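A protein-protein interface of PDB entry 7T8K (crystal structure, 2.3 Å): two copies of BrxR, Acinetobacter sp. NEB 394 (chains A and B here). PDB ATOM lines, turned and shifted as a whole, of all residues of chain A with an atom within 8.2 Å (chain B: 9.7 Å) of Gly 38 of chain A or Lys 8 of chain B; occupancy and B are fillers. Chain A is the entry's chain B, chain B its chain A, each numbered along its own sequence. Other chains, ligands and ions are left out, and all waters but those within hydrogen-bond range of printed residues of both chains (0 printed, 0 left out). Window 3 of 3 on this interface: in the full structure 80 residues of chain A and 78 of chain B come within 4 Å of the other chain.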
ATOM      1  N   GLU A  10     -18.856  36.632 -11.231  1.00  0.00           N
ATOM      2  CA  GLU A  10     -19.071  35.198 -11.079  1.00  0.00           C
ATOM      3  C   GLU A  10     -17.940  34.563 -10.283  1.00  0.00           C
ATOM      4  O   GLU A  10     -18.178  33.795  -9.345  1.00  0.00           O
ATOM      5  CB  GLU A  10     -19.204  34.533 -12.448  1.00  0.00           C
ATOM      6  CG  GLU A  10     -19.075  33.020 -12.388  1.00  0.00           C
ATOM      7  CD  GLU A  10     -19.791  32.326 -13.524  1.00  0.00           C
ATOM      8  OE1 GLU A  10     -20.091  31.122 -13.384  1.00  0.00           O
ATOM      9  OE2 GLU A  10     -20.047  32.981 -14.559  1.00  0.00           O
ATOM     10  N   ARG A  14     -17.769  32.689  -6.382  1.00  0.00           N
ATOM     11  CA  ARG A  14     -17.170  31.390  -6.099  1.00  0.00           C
ATOM     12  C   ARG A  14     -16.110  31.503  -5.008  1.00  0.00           C
ATOM     13  O   ARG A  14     -16.029  30.647  -4.117  1.00  0.00           O
ATOM     14  CB  ARG A  14     -16.588  30.801  -7.388  1.00  0.00           C
ATOM     15  CG  ARG A  14     -17.542  29.847  -8.109  1.00  0.00           C
ATOM     16  CD  ARG A  14     -17.593  30.081  -9.621  1.00  0.00           C
ATOM     17  NE  ARG A  14     -16.327  29.778 -10.287  1.00  0.00           N
ATOM     18  CZ  ARG A  14     -16.086  30.001 -11.575  1.00  0.00           C
ATOM     19  NH1 ARG A  14     -17.032  30.507 -12.353  1.00  0.00           N
ATOM     20  NH2 ARG A  14     -14.902  29.696 -12.093  1.00  0.00           N
ATOM     21  N   THR A  31     -17.030  19.062  -4.805  1.00  0.00           N
ATOM     22  CA  THR A  31     -18.367  18.595  -5.156  1.00  0.00           C
ATOM     23  C   THR A  31     -19.424  19.621  -4.778  1.00  0.00           C
ATOM     24  O   THR A  31     -20.392  19.829  -5.517  1.00  0.00           O
ATOM     25  CB  THR A  31     -18.654  17.261  -4.467  1.00  0.00           C
ATOM     26  OG1 THR A  31     -17.604  16.331  -4.764  1.00  0.00           O
ATOM     27  CG2 THR A  31     -19.989  16.689  -4.936  1.00  0.00           C
ATOM     28  N   ARG A  32     -19.248  20.282  -3.634  1.00  0.00           N
ATOM     29  CA  ARG A  32     -20.209  21.294  -3.219  1.00  0.00           C
ATOM     30  C   ARG A  32     -20.234  22.446  -4.213  1.00  0.00           C
ATOM     31  O   ARG A  32     -21.306  22.888  -4.643  1.00  0.00           O
ATOM     32  CB  ARG A  32     -19.863  21.791  -1.813  1.00  0.00           C
ATOM     33  CG  ARG A  32     -20.925  22.657  -1.156  1.00  0.00           C
ATOM     34  CD  ARG A  32     -22.119  21.837  -0.690  1.00  0.00           C
ATOM     35  NE  ARG A  32     -22.949  22.571   0.263  1.00  0.00           N
ATOM     36  CZ  ARG A  32     -22.634  22.769   1.541  1.00  0.00           C
ATOM     37  NH1 ARG A  32     -21.498  22.290   2.038  1.00  0.00           N
ATOM     38  NH2 ARG A  32     -23.455  23.452   2.325  1.00  0.00           N
ATOM     39  N   LEU A  33     -19.054  22.931  -4.610  1.00  0.00           N
ATOM     40  CA  LEU A  33     -18.995  24.002  -5.600  1.00  0.00           C
ATOM     41  C   LEU A  33     -19.591  23.547  -6.920  1.00  0.00           C
ATOM     42  O   LEU A  33     -20.265  24.323  -7.608  1.00  0.00           O
ATOM     43  CB  LEU A  33     -17.550  24.458  -5.812  1.00  0.00           C
ATOM     44  CG  LEU A  33     -16.833  25.323  -4.774  1.00  0.00           C
ATOM     45  CD1 LEU A  33     -17.748  26.397  -4.207  1.00  0.00           C
ATOM     46  CD2 LEU A  33     -16.255  24.463  -3.668  1.00  0.00           C
ATOM     47  N   MET A  34     -19.364  22.283  -7.284  1.00  0.00           N
ATOM     48  CA  MET A  34     -19.946  21.759  -8.514  1.00  0.00           C
ATOM     49  C   MET A  34     -21.463  21.802  -8.441  1.00  0.00           C
ATOM     50  O   MET A  34     -22.124  22.325  -9.343  1.00  0.00           O
ATOM     51  CB  MET A  34     -19.456  20.332  -8.764  1.00  0.00           C
ATOM     52  CG  MET A  34     -17.982  20.221  -9.135  1.00  0.00           C
ATOM     53  SD  MET A  34     -17.385  18.518  -9.031  1.00  0.00           S
ATOM     54  CE  MET A  34     -18.541  17.715 -10.145  1.00  0.00           C
ATOM     55  N   ASN A  35     -22.030  21.309  -7.339  1.00  0.00           N
ATOM     56  CA  ASN A  35     -23.479  21.340  -7.174  1.00  0.00           C
ATOM     57  C   ASN A  35     -24.019  22.766  -7.111  1.00  0.00           C
ATOM     58  O   ASN A  35     -25.155  23.014  -7.528  1.00  0.00           O
ATOM     59  CB  ASN A  35     -23.874  20.565  -5.920  1.00  0.00           C
ATOM     60  CG  ASN A  35     -23.910  19.067  -6.152  1.00  0.00           C
ATOM     61  OD1 ASN A  35     -23.150  18.535  -6.965  1.00  0.00           O
ATOM     62  ND2 ASN A  35     -24.793  18.379  -5.441  1.00  0.00           N
ATOM     63  N   TRP A  36     -23.233  23.713  -6.595  1.00  0.00           N
ATOM     64  CA  TRP A  36     -23.740  25.072  -6.431  1.00  0.00           C
ATOM     65  C   TRP A  36     -23.708  25.857  -7.740  1.00  0.00           C
ATOM     66  O   TRP A  36     -24.668  26.566  -8.061  1.00  0.00           O
ATOM     67  CB  TRP A  36     -22.937  25.813  -5.357  1.00  0.00           C
ATOM     68  CG  TRP A  36     -23.349  25.497  -3.949  1.00  0.00           C
ATOM     69  CD1 TRP A  36     -24.256  24.560  -3.551  1.00  0.00           C
ATOM     70  CD2 TRP A  36     -22.871  26.126  -2.752  1.00  0.00           C
ATOM     71  NE1 TRP A  36     -24.371  24.563  -2.181  1.00  0.00           N
ATOM     72  CE2 TRP A  36     -23.532  25.517  -1.666  1.00  0.00           C
ATOM     73  CE3 TRP A  36     -21.952  27.149  -2.493  1.00  0.00           C
ATOM     74  CZ2 TRP A  36     -23.302  25.893  -0.344  1.00  0.00           C
ATOM     75  CZ3 TRP A  36     -21.724  27.521  -1.176  1.00  0.00           C
ATOM     76  CH2 TRP A  36     -22.397  26.894  -0.121  1.00  0.00           C
ATOM     77  N   PHE A  37     -22.620  25.750  -8.505  1.00  0.00           N
ATOM     78  CA  PHE A  37     -22.412  26.598  -9.671  1.00  0.00           C
ATOM     79  C   PHE A  37     -22.451  25.866 -11.011  1.00  0.00           C
ATOM     80  O   PHE A  37     -22.253  26.515 -12.045  1.00  0.00           O
ATOM     81  CB  PHE A  37     -21.083  27.351  -9.537  1.00  0.00           C
ATOM     82  CG  PHE A  37     -21.010  28.245  -8.327  1.00  0.00           C
ATOM     83  CD1 PHE A  37     -21.632  29.481  -8.326  1.00  0.00           C
ATOM     84  CD2 PHE A  37     -20.324  27.847  -7.192  1.00  0.00           C
ATOM     85  CE1 PHE A  37     -21.569  30.304  -7.215  1.00  0.00           C
ATOM     86  CE2 PHE A  37     -20.256  28.661  -6.083  1.00  0.00           C
ATOM     87  CZ  PHE A  37     -20.879  29.892  -6.091  1.00  0.00           C
ATOM     88  N   GLY A  38     -22.707  24.556 -11.047  1.00  0.00           N
ATOM     89  CA  GLY A  38     -22.733  23.855 -12.319  1.00  0.00           C
ATOM     90  C   GLY A  38     -21.378  23.687 -12.970  1.00  0.00           C
ATOM     91  O   GLY A  38     -21.291  23.662 -14.201  1.00  0.00           O
ATOM     92  N   LEU A  39     -20.318  23.575 -12.179  1.00  0.00           N
ATOM     93  CA  LEU A  39     -18.955  23.524 -12.682  1.00  0.00           C
ATOM     94  C   LEU A  39     -18.445  22.093 -12.791  1.00  0.00           C
ATOM     95  O   LEU A  39     -18.935  21.169 -12.136  1.00  0.00           O
ATOM     96  CB  LEU A  39     -18.005  24.307 -11.774  1.00  0.00           C
ATOM     97  CG  LEU A  39     -18.176  25.811 -11.600  1.00  0.00           C
ATOM     98  CD1 LEU A  39     -17.046  26.331 -10.729  1.00  0.00           C
ATOM     99  CD2 LEU A  39     -18.183  26.505 -12.950  1.00  0.00           C
ATOM    100  N   SER A  40     -17.424  21.931 -13.625  1.00  0.00           N
ATOM    101  CA  SER A  40     -16.650  20.706 -13.618  1.00  0.00           C
ATOM    102  C   SER A  40     -15.781  20.674 -12.368  1.00  0.00           C
ATOM    103  O   SER A  40     -15.434  21.715 -11.803  1.00  0.00           O
ATOM    104  CB  SER A  40     -15.774  20.623 -14.868  1.00  0.00           C
ATOM    105  OG  SER A  40     -14.712  21.559 -14.790  1.00  0.00           O
ATOM    106  N   ARG A  41     -15.434  19.463 -11.928  1.00  0.00           N
ATOM    107  CA  ARG A  41     -14.520  19.342 -10.797  1.00  0.00           C
ATOM    108  C   ARG A  41     -13.207  20.061 -11.068  1.00  0.00           C
ATOM    109  O   ARG A  41     -12.593  20.607 -10.144  1.00  0.00           O
ATOM    110  CB  ARG A  41     -14.258  17.872 -10.471  1.00  0.00           C
ATOM    111  CG  ARG A  41     -13.170  17.669  -9.427  1.00  0.00           C
ATOM    112  CD  ARG A  41     -13.105  16.221  -8.960  1.00  0.00           C
ATOM    113  NE  ARG A  41     -12.432  15.360  -9.929  1.00  0.00           N
ATOM    114  CZ  ARG A  41     -11.114  15.232 -10.032  1.00  0.00           C
ATOM    115  NH1 ARG A  41     -10.315  15.902  -9.219  1.00  0.00           N
ATOM    116  NH2 ARG A  41     -10.596  14.421 -10.944  1.00  0.00           N
ATOM    117  N   GLN A  43     -12.620  22.851 -12.874  1.00  0.00           N
ATOM    118  CA  GLN A  43     -12.727  24.287 -12.636  1.00  0.00           C
ATOM    119  C   GLN A  43     -12.878  24.587 -11.148  1.00  0.00           C
ATOM    120  O   GLN A  43     -12.255  25.523 -10.636  1.00  0.00           O
ATOM    121  CB  GLN A  43     -13.898  24.873 -13.423  1.00  0.00           C
ATOM    122  CG  GLN A  43     -13.963  26.399 -13.402  1.00  0.00           C
ATOM    123  CD  GLN A  43     -12.652  27.045 -13.801  1.00  0.00           C
ATOM    124  OE1 GLN A  43     -12.186  26.884 -14.930  1.00  0.00           O
ATOM    125  NE2 GLN A  43     -12.047  27.782 -12.874  1.00  0.00           N
ATOM    126  N   ALA A  44     -13.683  23.796 -10.433  1.00  0.00           N
ATOM    127  CA  ALA A  44     -13.827  24.006  -8.993  1.00  0.00           C
ATOM    128  C   ALA A  44     -12.492  23.827  -8.282  1.00  0.00           C
ATOM    129  O   ALA A  44     -12.150  24.599  -7.376  1.00  0.00           O
ATOM    130  CB  ALA A  44     -14.879  23.053  -8.425  1.00  0.00           C
ATOM    131  N   ALA B   6     -31.357  23.966 -17.572  1.00  0.00           N
ATOM    132  CA  ALA B   6     -30.016  23.396 -17.453  1.00  0.00           C
ATOM    133  C   ALA B   6     -28.949  24.488 -17.336  1.00  0.00           C
ATOM    134  O   ALA B   6     -27.755  24.205 -17.443  1.00  0.00           O
ATOM    135  CB  ALA B   6     -29.713  22.473 -18.630  1.00  0.00           C
ATOM    136  N   ASP B   7     -29.379  25.731 -17.128  1.00  0.00           N
ATOM    137  CA  ASP B   7     -28.459  26.864 -17.119  1.00  0.00           C
ATOM    138  C   ASP B   7     -27.687  26.951 -15.809  1.00  0.00           C
ATOM    139  O   ASP B   7     -28.212  26.646 -14.734  1.00  0.00           O
ATOM    140  CB  ASP B   7     -29.226  28.171 -17.335  1.00  0.00           C
ATOM    141  CG  ASP B   7     -29.192  28.641 -18.775  1.00  0.00           C
ATOM    142  OD1 ASP B   7     -30.116  29.376 -19.181  1.00  0.00           O
ATOM    143  OD2 ASP B   7     -28.243  28.279 -19.501  1.00  0.00           O
ATOM    144  N   LYS B   8     -26.429  27.376 -15.909  1.00  0.00           N
ATOM    145  CA  LYS B   8     -25.577  27.524 -14.739  1.00  0.00           C
ATOM    146  C   LYS B   8     -26.111  28.628 -13.827  1.00  0.00           C
ATOM    147  O   LYS B   8     -26.808  29.551 -14.257  1.00  0.00           O
ATOM    148  CB  LYS B   8     -24.135  27.819 -15.155  1.00  0.00           C
ATOM    149  CG  LYS B   8     -23.408  26.626 -15.755  1.00  0.00           C
ATOM    150  N   HIS B   9     -25.736  28.540 -12.550  1.00  0.00           N
ATOM    151  CA  HIS B   9     -26.268  29.455 -11.545  1.00  0.00           C
ATOM    152  C   HIS B   9     -26.048  30.918 -11.917  1.00  0.00           C
ATOM    153  O   HIS B   9     -26.937  31.753 -11.719  1.00  0.00           O
ATOM    154  CB  HIS B   9     -25.642  29.150 -10.183  1.00  0.00           C
ATOM    155  CG  HIS B   9     -26.066  30.091  -9.100  1.00  0.00           C
ATOM    156  ND1 HIS B   9     -27.346  30.108  -8.586  1.00  0.00           N
ATOM    157  CD2 HIS B   9     -25.383  31.053  -8.434  1.00  0.00           C
ATOM    158  CE1 HIS B   9     -27.431  31.036  -7.650  1.00  0.00           C
ATOM    159  NE2 HIS B   9     -26.255  31.624  -7.538  1.00  0.00           N
ATOM    160  N   GLU B  10     -24.872  31.250 -12.456  1.00  0.00           N
ATOM    161  CA  GLU B  10     -24.585  32.636 -12.820  1.00  0.00           C
ATOM    162  C   GLU B  10     -25.577  33.159 -13.853  1.00  0.00           C
ATOM    163  O   GLU B  10     -26.130  34.254 -13.700  1.00  0.00           O
ATOM    164  CB  GLU B  10     -23.150  32.755 -13.335  1.00  0.00           C
ATOM    165  CG  GLU B  10     -22.701  34.176 -13.674  1.00  0.00           C
ATOM    166  CD  GLU B  10     -22.577  35.081 -12.454  1.00  0.00           C
ATOM    167  OE1 GLU B  10     -22.795  34.606 -11.317  1.00  0.00           O
ATOM    168  OE2 GLU B  10     -22.245  36.270 -12.636  1.00  0.00           O
ATOM    169  N   VAL B  11     -25.805  32.399 -14.927  1.00  0.00           N
ATOM    170  CA  VAL B  11     -26.798  32.812 -15.914  1.00  0.00           C
ATOM    171  C   VAL B  11     -28.164  32.913 -15.258  1.00  0.00           C
ATOM    172  O   VAL B  11     -28.955  33.818 -15.556  1.00  0.00           O
ATOM    173  CB  VAL B  11     -26.821  31.843 -17.112  1.00  0.00           C
ATOM    174  CG1 VAL B  11     -27.893  32.272 -18.107  1.00  0.00           C
ATOM    175  CG2 VAL B  11     -25.457  31.790 -17.788  1.00  0.00           C
ATOM    176  N   LEU B  12     -28.460  31.987 -14.348  1.00  0.00           N
ATOM    177  CA  LEU B  12     -29.728  32.029 -13.633  1.00  0.00           C
ATOM    178  C   LEU B  12     -29.872  33.315 -12.832  1.00  0.00           C
ATOM    179  O   LEU B  12     -30.964  33.886 -12.758  1.00  0.00           O
ATOM    180  CB  LEU B  12     -29.846  30.813 -12.720  1.00  0.00           C
ATOM    181  CG  LEU B  12     -31.206  30.123 -12.722  1.00  0.00           C
ATOM    182  CD1 LEU B  12     -31.833  30.209 -14.105  1.00  0.00           C
ATOM    183  CD2 LEU B  12     -31.046  28.672 -12.290  1.00  0.00           C
ATOM    184  N   LEU B  13     -28.789  33.780 -12.206  1.00  0.00           N
ATOM    185  CA  LEU B  13     -28.879  35.030 -11.459  1.00  0.00           C
ATOM    186  C   LEU B  13     -29.173  36.192 -12.396  1.00  0.00           C
ATOM    187  O   LEU B  13     -29.923  37.108 -12.046  1.00  0.00           O
ATOM    188  CB  LEU B  13     -27.593  35.285 -10.676  1.00  0.00           C
ATOM    189  CG  LEU B  13     -27.476  34.602  -9.313  1.00  0.00           C
ATOM    190  CD1 LEU B  13     -26.081  34.795  -8.737  1.00  0.00           C
ATOM    191  CD2 LEU B  13     -28.541  35.110  -8.344  1.00  0.00           C
ATOM    192  N   ARG B  14     -28.609  36.164 -13.602  1.00  0.00           N
ATOM    193  CA  ARG B  14     -28.886  37.224 -14.562  1.00  0.00           C
ATOM    194  C   ARG B  14     -30.326  37.152 -15.060  1.00  0.00           C
ATOM    195  O   ARG B  14     -30.984  38.186 -15.229  1.00  0.00           O
ATOM    196  CB  ARG B  14     -27.887  37.151 -15.714  1.00  0.00           C
ATOM    197  CG  ARG B  14     -26.584  37.881 -15.401  1.00  0.00           C
ATOM    198  CD  ARG B  14     -25.348  37.083 -15.791  1.00  0.00           C
ATOM    199  NE  ARG B  14     -25.196  36.989 -17.239  1.00  0.00           N
ATOM    200  CZ  ARG B  14     -24.391  36.124 -17.848  1.00  0.00           C
ATOM    201  NH1 ARG B  14     -23.641  35.294 -17.133  1.00  0.00           N
ATOM    202  NH2 ARG B  14     -24.319  36.102 -19.171  1.00  0.00           N
ATOM    203  N   MET B  15     -30.832  35.941 -15.310  1.00  0.00           N
ATOM    204  CA  MET B  15     -32.236  35.797 -15.682  1.00  0.00           C
ATOM    205  C   MET B  15     -33.146  36.322 -14.577  1.00  0.00           C
ATOM    206  O   MET B  15     -34.092  37.074 -14.840  1.00  0.00           O
ATOM    207  CB  MET B  15     -32.554  34.333 -15.996  1.00  0.00           C
ATOM    208  CG  MET B  15     -31.699  33.716 -17.104  1.00  0.00           C
ATOM    209  SD  MET B  15     -31.944  34.471 -18.728  1.00  0.00           S
ATOM    210  CE  MET B  15     -30.622  35.681 -18.730  1.00  0.00           C
ATOM    211  N   ARG B  16     -32.880  35.915 -13.330  1.00  0.00           N
ATOM    212  CA  ARG B  16     -33.633  36.420 -12.187  1.00  0.00           C
ATOM    213  C   ARG B  16     -33.576  37.937 -12.121  1.00  0.00           C
ATOM    214  O   ARG B  16     -34.583  38.588 -11.831  1.00  0.00           O
ATOM    215  CB  ARG B  16     -33.092  35.831 -10.881  1.00  0.00           C
ATOM    216  CG  ARG B  16     -33.365  34.351 -10.651  1.00  0.00           C
ATOM    217  CD  ARG B  16     -33.254  34.007  -9.159  1.00  0.00           C
ATOM    218  NE  ARG B  16     -34.420  33.274  -8.667  1.00  0.00           N
ATOM    219  CZ  ARG B  16     -35.109  33.595  -7.575  1.00  0.00           C
ATOM    220  NH1 ARG B  16     -34.761  34.646  -6.842  1.00  0.00           N
ATOM    221  NH2 ARG B  16     -36.153  32.862  -7.210  1.00  0.00           N
ATOM    222  N   ARG B  50     -32.013  36.049 -24.319  1.00  0.00           N
ATOM    223  CA  ARG B  50     -32.161  34.712 -23.752  1.00  0.00           C
ATOM    224  C   ARG B  50     -33.381  34.643 -22.848  1.00  0.00           C
ATOM    225  O   ARG B  50     -34.172  33.698 -22.925  1.00  0.00           O
ATOM    226  CB  ARG B  50     -30.900  34.327 -22.980  1.00  0.00           C
ATOM    227  CG  ARG B  50     -30.823  32.856 -22.603  1.00  0.00           C
ATOM    228  CD  ARG B  50     -29.552  32.573 -21.818  1.00  0.00           C
ATOM    229  NE  ARG B  50     -29.339  31.150 -21.569  1.00  0.00           N
ATOM    230  CZ  ARG B  50     -29.164  30.241 -22.524  1.00  0.00           C
ATOM    231  NH1 ARG B  50     -29.178  30.608 -23.797  1.00  0.00           N
ATOM    232  NH2 ARG B  50     -28.974  28.967 -22.206  1.00  0.00           N
ATOM    233  N   TYR B  55     -37.089  31.714 -21.469  1.00  0.00           N
ATOM    234  CA  TYR B  55     -37.685  31.659 -20.140  1.00  0.00           C
ATOM    235  C   TYR B  55     -39.099  32.213 -20.116  1.00  0.00           C
ATOM    236  O   TYR B  55     -40.018  31.549 -19.633  1.00  0.00           O
ATOM    237  CB  TYR B  55     -36.801  32.419 -19.140  1.00  0.00           C
ATOM    238  CG  TYR B  55     -35.564  31.644 -18.741  1.00  0.00           C
ATOM    239  CD1 TYR B  55     -34.377  31.785 -19.447  1.00  0.00           C
ATOM    240  CD2 TYR B  55     -35.592  30.756 -17.676  1.00  0.00           C
ATOM    241  CE1 TYR B  55     -33.249  31.069 -19.098  1.00  0.00           C
ATOM    242  CE2 TYR B  55     -34.466  30.037 -17.318  1.00  0.00           C
ATOM    243  CZ  TYR B  55     -33.299  30.198 -18.032  1.00  0.00           C
ATOM    244  OH  TYR B  55     -32.180  29.486 -17.673  1.00  0.00           O
ATOM    245  N   LEU B  79     -39.470  32.789 -12.894  1.00  0.00           N
ATOM    246  CA  LEU B  79     -38.395  32.288 -12.048  1.00  0.00           C
ATOM    247  C   LEU B  79     -38.513  32.723 -10.597  1.00  0.00           C
ATOM    248  O   LEU B  79     -37.717  32.270  -9.766  1.00  0.00           O
ATOM    249  CB  LEU B  79     -37.025  32.721 -12.591  1.00  0.00           C
ATOM    250  CG  LEU B  79     -36.703  32.215 -13.998  1.00  0.00           C
ATOM    251  CD1 LEU B  79     -35.466  32.904 -14.551  1.00  0.00           C
ATOM    252  CD2 LEU B  79     -36.529  30.708 -13.977  1.00  0.00           C
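The side-chain carboxylate of Glu 10 of chain A lies within salt-bridge range of the guanidinium group of Arg 14 of chain A (3.3 Å).
Glu 10 of chain B touches Glu 10 of chain A.
Trp 36 of chain A touches His 9 of chain B (O to CB, 3.5 Å).
Lys 8 of chain B touches Phe 37 of chain A.
Lys 8 of chain B touches Gly 38 of chain A (CG to O, 3.96 Å).
Gly 38 of chain A touches just one residue of chain B: Lys 8 (3.96 Å).
Lys 8 of chain B touches just these residues of chain A: Phe 37 and Gly 38.
No residue of chain B comes within 4 Å of Leu 39 of chain A.
Printed residues of chain B within 4 Å of Glu 10 of chain A: Glu 10.
Printed residues of chain A within 4 Å of Glu 10 of chain B: Glu 10 (3.0 Å).
Of the printed residues of chain B, Trp 36 of chain A touches His 9.
Of the 14 printed residues of chain B, 3 touch a printed residue of chain A.
Hydrophobic or aromatic side chains of chain B that line the printed part of chain A: His 9.
Of the 15 printed residues of chain A, 4 touch a printed residue of chain B.
Among the printed residues, 4 pairs touch across the chains.
Glu 10 of chain A touches its own counterpart, Glu 10 of chain B.
Positions printed for both chains: 10 and 14.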
